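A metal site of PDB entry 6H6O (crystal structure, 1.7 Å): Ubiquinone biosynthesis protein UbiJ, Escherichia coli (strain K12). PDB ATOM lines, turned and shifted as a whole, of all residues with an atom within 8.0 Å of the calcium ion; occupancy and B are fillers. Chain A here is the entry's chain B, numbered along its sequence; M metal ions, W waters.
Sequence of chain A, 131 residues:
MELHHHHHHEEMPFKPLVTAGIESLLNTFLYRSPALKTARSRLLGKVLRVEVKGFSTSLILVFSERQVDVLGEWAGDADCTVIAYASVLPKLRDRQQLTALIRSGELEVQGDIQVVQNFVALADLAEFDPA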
ATOM      1  N   PHE A  29     -10.394  -2.445  10.257  1.00  0.00           N
ATOM      2  CA  PHE A  29     -10.942  -1.381   9.417  1.00  0.00           C
ATOM      3  C   PHE A  29     -12.328  -1.737   8.801  1.00  0.00           C
ATOM      4  O   PHE A  29     -13.240  -0.899   8.845  1.00  0.00           O
ATOM      5  CB  PHE A  29      -9.929  -0.984   8.330  1.00  0.00           C
ATOM      6  CG  PHE A  29     -10.327   0.190   7.450  1.00  0.00           C
ATOM      7  CD1 PHE A  29     -10.508   1.455   7.982  1.00  0.00           C
ATOM      8  CD2 PHE A  29     -10.480   0.015   6.074  1.00  0.00           C
ATOM      9  CE1 PHE A  29     -10.850   2.540   7.158  1.00  0.00           C
ATOM     10  CE2 PHE A  29     -10.867   1.097   5.254  1.00  0.00           C
ATOM     11  CZ  PHE A  29     -11.024   2.352   5.804  1.00  0.00           C
ATOM     12  N   ARG A  93     -10.215   3.738  -1.238  1.00  0.00           N
ATOM     13  CA  ARG A  93     -11.306   3.933  -0.258  1.00  0.00           C
ATOM     14  C   ARG A  93     -12.298   4.989  -0.784  1.00  0.00           C
ATOM     15  O   ARG A  93     -13.057   5.583  -0.010  1.00  0.00           O
ATOM     16  CB  ARG A  93     -10.762   4.321   1.121  1.00  0.00           C
ATOM     17  CG  ARG A  93      -9.768   3.327   1.727  1.00  0.00           C
ATOM     18  CD  ARG A  93      -8.425   4.001   1.917  1.00  0.00           C
ATOM     19  NE  ARG A  93      -8.450   4.971   3.019  1.00  0.00           N
ATOM     20  CZ  ARG A  93      -7.493   5.862   3.246  1.00  0.00           C
ATOM     21  NH1 ARG A  93      -6.445   5.951   2.442  1.00  0.00           N
ATOM     22  NH2 ARG A  93      -7.595   6.699   4.269  1.00  0.00           N
ATOM     23  N   ASP A  94     -12.295   5.223  -2.101  1.00  0.00           N
ATOM     24  CA  ASP A  94     -13.191   6.178  -2.744  1.00  0.00           C
ATOM     25  C   ASP A  94     -13.752   5.530  -4.012  1.00  0.00           C
ATOM     26  O   ASP A  94     -13.046   5.375  -5.004  1.00  0.00           O
ATOM     27  CB  ASP A  94     -12.445   7.505  -3.032  1.00  0.00           C
ATOM     28  CG  ASP A  94     -13.276   8.628  -3.636  1.00  0.00           C
ATOM     29  OD1 ASP A  94     -14.522   8.502  -3.662  1.00  0.00           O
ATOM     30  OD2 ASP A  94     -12.678   9.650  -4.055  1.00  0.00           O
ATOM     31  N   ARG A  95     -15.028   5.110  -3.949  1.00  0.00           N
ATOM     32  CA  ARG A  95     -15.668   4.398  -5.054  1.00  0.00           C
ATOM     33  C   ARG A  95     -15.793   5.195  -6.340  1.00  0.00           C
ATOM     34  O   ARG A  95     -15.726   4.612  -7.419  1.00  0.00           O
ATOM     35  CB  ARG A  95     -17.036   3.800  -4.672  1.00  0.00           C
ATOM     36  CG  ARG A  95     -17.218   2.414  -5.288  1.00  0.00           C
ATOM     37  CD  ARG A  95     -18.564   2.158  -5.944  1.00  0.00           C
ATOM     38  NE  ARG A  95     -18.787   0.719  -6.086  1.00  0.00           N
ATOM     39  CZ  ARG A  95     -19.962   0.143  -6.281  1.00  0.00           C
ATOM     40  NH1 ARG A  95     -21.058   0.879  -6.392  1.00  0.00           N
ATOM     41  NH2 ARG A  95     -20.063  -1.176  -6.363  1.00  0.00           N
ATOM     42  N   VAL A 120     -13.818  -1.500  -2.826  1.00  0.00           N
ATOM     43  CA  VAL A 120     -13.661  -0.046  -2.738  1.00  0.00           C
ATOM     44  C   VAL A 120     -14.928   0.585  -2.141  1.00  0.00           C
ATOM     45  O   VAL A 120     -14.817   1.420  -1.247  1.00  0.00           O
ATOM     46  CB  VAL A 120     -13.240   0.576  -4.090  1.00  0.00           C
ATOM     47  CG1 VAL A 120     -13.194   2.094  -4.006  1.00  0.00           C
ATOM     48  CG2 VAL A 120     -11.874   0.052  -4.530  1.00  0.00           C
ATOM     49  N   ALA A 121     -16.134   0.128  -2.550  1.00  0.00           N
ATOM     50  CA  ALA A 121     -17.407   0.604  -2.000  1.00  0.00           C
ATOM     51  C   ALA A 121     -17.452   0.314  -0.493  1.00  0.00           C
ATOM     52  O   ALA A 121     -17.797   1.202   0.279  1.00  0.00           O
ATOM     53  CB  ALA A 121     -18.572  -0.091  -2.716  1.00  0.00           C
ATOM     54  N   LEU A 122     -17.016  -0.919  -0.067  1.00  0.00           N
ATOM     55  CA  LEU A 122     -16.979  -1.301   1.341  1.00  0.00           C
ATOM     56  C   LEU A 122     -15.978  -0.425   2.113  1.00  0.00           C
ATOM     57  O   LEU A 122     -16.324   0.108   3.177  1.00  0.00           O
ATOM     58  CB  LEU A 122     -16.655  -2.809   1.503  1.00  0.00           C
ATOM     59  CG  LEU A 122     -16.297  -3.281   2.912  1.00  0.00           C
ATOM     60  CD1 LEU A 122     -17.468  -3.069   3.920  1.00  0.00           C
ATOM     61  CD2 LEU A 122     -15.817  -4.734   2.893  1.00  0.00           C
ATOM     62  N   ALA A 123     -14.740  -0.296   1.572  1.00  0.00           N
ATOM     63  CA  ALA A 123     -13.690   0.551   2.160  1.00  0.00           C
ATOM     64  C   ALA A 123     -14.182   2.032   2.311  1.00  0.00           C
ATOM     65  O   ALA A 123     -13.934   2.663   3.353  1.00  0.00           O
ATOM     66  CB  ALA A 123     -12.441   0.473   1.296  1.00  0.00           C
ATOM     67  N   ASP A 124     -14.931   2.548   1.334  1.00  0.00           N
ATOM     68  CA  ASP A 124     -15.513   3.896   1.380  1.00  0.00           C
ATOM     69  C   ASP A 124     -16.531   4.014   2.511  1.00  0.00           C
ATOM     70  O   ASP A 124     -16.445   4.942   3.318  1.00  0.00           O
ATOM     71  CB  ASP A 124     -16.152   4.242   0.037  1.00  0.00           C
ATOM     72  CG  ASP A 124     -16.401   5.712  -0.226  1.00  0.00           C
ATOM     73  OD1 ASP A 124     -16.146   6.547   0.689  1.00  0.00           O
ATOM     74  OD2 ASP A 124     -16.820   6.041  -1.351  1.00  0.00           O
ATOM     75  N   LEU A 125     -17.433   3.013   2.639  1.00  0.00           N
ATOM     76  CA  LEU A 125     -18.446   2.983   3.696  1.00  0.00           C
ATOM     77  C   LEU A 125     -17.822   2.786   5.076  1.00  0.00           C
ATOM     78  O   LEU A 125     -18.361   3.314   6.058  1.00  0.00           O
ATOM     79  CB  LEU A 125     -19.509   1.915   3.414  1.00  0.00           C
ATOM     80  CG  LEU A 125     -20.444   2.262   2.224  1.00  0.00           C
ATOM     81  CD1 LEU A 125     -21.328   1.089   1.865  1.00  0.00           C
ATOM     82  CD2 LEU A 125     -21.296   3.543   2.493  1.00  0.00           C
ATOM     83  N   ALA A 126     -16.679   2.095   5.149  1.00  0.00           N
ATOM     84  CA  ALA A 126     -15.972   1.891   6.428  1.00  0.00           C
ATOM     85  C   ALA A 126     -15.335   3.170   6.980  1.00  0.00           C
ATOM     86  O   ALA A 126     -14.936   3.180   8.149  1.00  0.00           O
ATOM     87  CB  ALA A 126     -14.890   0.831   6.236  1.00  0.00           C
ATOM     88  N   GLU A 127     -15.244   4.261   6.195  1.00  0.00           N
ATOM     89  CA  GLU A 127     -14.526   5.448   6.649  1.00  0.00           C
ATOM     90  C   GLU A 127     -15.217   6.789   6.414  1.00  0.00           C
ATOM     91  O   GLU A 127     -15.648   7.086   5.300  1.00  0.00           O
ATOM     92  CB  GLU A 127     -13.158   5.422   5.937  1.00  0.00           C
ATOM     93  CG  GLU A 127     -12.247   6.626   6.095  1.00  0.00           C
ATOM     94  CD  GLU A 127     -11.018   6.468   5.228  1.00  0.00           C
ATOM     95  OE1 GLU A 127      -9.919   6.258   5.791  1.00  0.00           O
ATOM     96  OE2 GLU A 127     -11.155   6.465   3.983  1.00  0.00           O
ATOM     97  N   PHE A 128     -15.268   7.617   7.476  1.00  0.00           N
ATOM     98  CA  PHE A 128     -15.785   8.987   7.398  1.00  0.00           C
ATOM     99  C   PHE A 128     -14.716   9.792   6.626  1.00  0.00           C
ATOM    100  O   PHE A 128     -13.529   9.625   6.904  1.00  0.00           O
ATOM    101  CB  PHE A 128     -15.954   9.586   8.823  1.00  0.00           C
ATOM    102  CG  PHE A 128     -17.205   9.143   9.553  1.00  0.00           C
ATOM    103  CD1 PHE A 128     -18.442   9.721   9.269  1.00  0.00           C
ATOM    104  CD2 PHE A 128     -17.133   8.166  10.541  1.00  0.00           C
ATOM    105  CE1 PHE A 128     -19.594   9.314   9.955  1.00  0.00           C
ATOM    106  CE2 PHE A 128     -18.285   7.759  11.227  1.00  0.00           C
ATOM    107  CZ  PHE A 128     -19.505   8.331  10.916  1.00  0.00           C
ATOM    108  N   ASP A 129     -15.132  10.602   5.628  1.00  0.00           N
ATOM    109  CA  ASP A 129     -14.211  11.380   4.785  1.00  0.00           C
ATOM    110  C   ASP A 129     -13.563  12.551   5.525  1.00  0.00           C
ATOM    111  O   ASP A 129     -14.108  13.058   6.510  1.00  0.00           O
ATOM    112  CB  ASP A 129     -14.920  11.867   3.512  1.00  0.00           C
ATOM    113  CG  ASP A 129     -15.263  10.783   2.490  1.00  0.00           C
ATOM    114  OD1 ASP A 129     -15.241   9.581   2.847  1.00  0.00           O
ATOM    115  OD2 ASP A 129     -15.588  11.155   1.344  1.00  0.00           O
HETATM  116 CA    CA M   1     -15.681   7.107   2.967  1.00  0.00          CA
HETATM  117  O   HOH W   1     -13.434   6.810   2.388  1.00  0.00           O
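The calcium ion is bound by the backbone carbonyl oxygen (O) of Asp 124 (2.3 Å), the backbone carbonyl oxygen (O) of Glu 127 (2.3 Å), water W1 (2.3 Å), the side-chain carboxylate (OD1) of Asp 124 (2.4 Å) and the side-chain carboxylate (OD1) of Asp 129 (2.5 Å).
The calcium ion has five donor atoms within binding distance.
NH2 of Arg 93 lies within salt-bridge range of OE1 of Glu 127.
OD2 of Asp 124 sits at hydrogen-bond distance from N of Arg 95 (3.3 Å).
Within 4 Å of the calcium ion: Asp 124, Glu 127 and Asp 129.
Water W1 lies within hydrogen-bond range of the backbone carbonyl oxygen (O) of Arg 93 (2.7 Å) and the side-chain carboxylate (OE2) of Glu 127 (2.8 Å).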
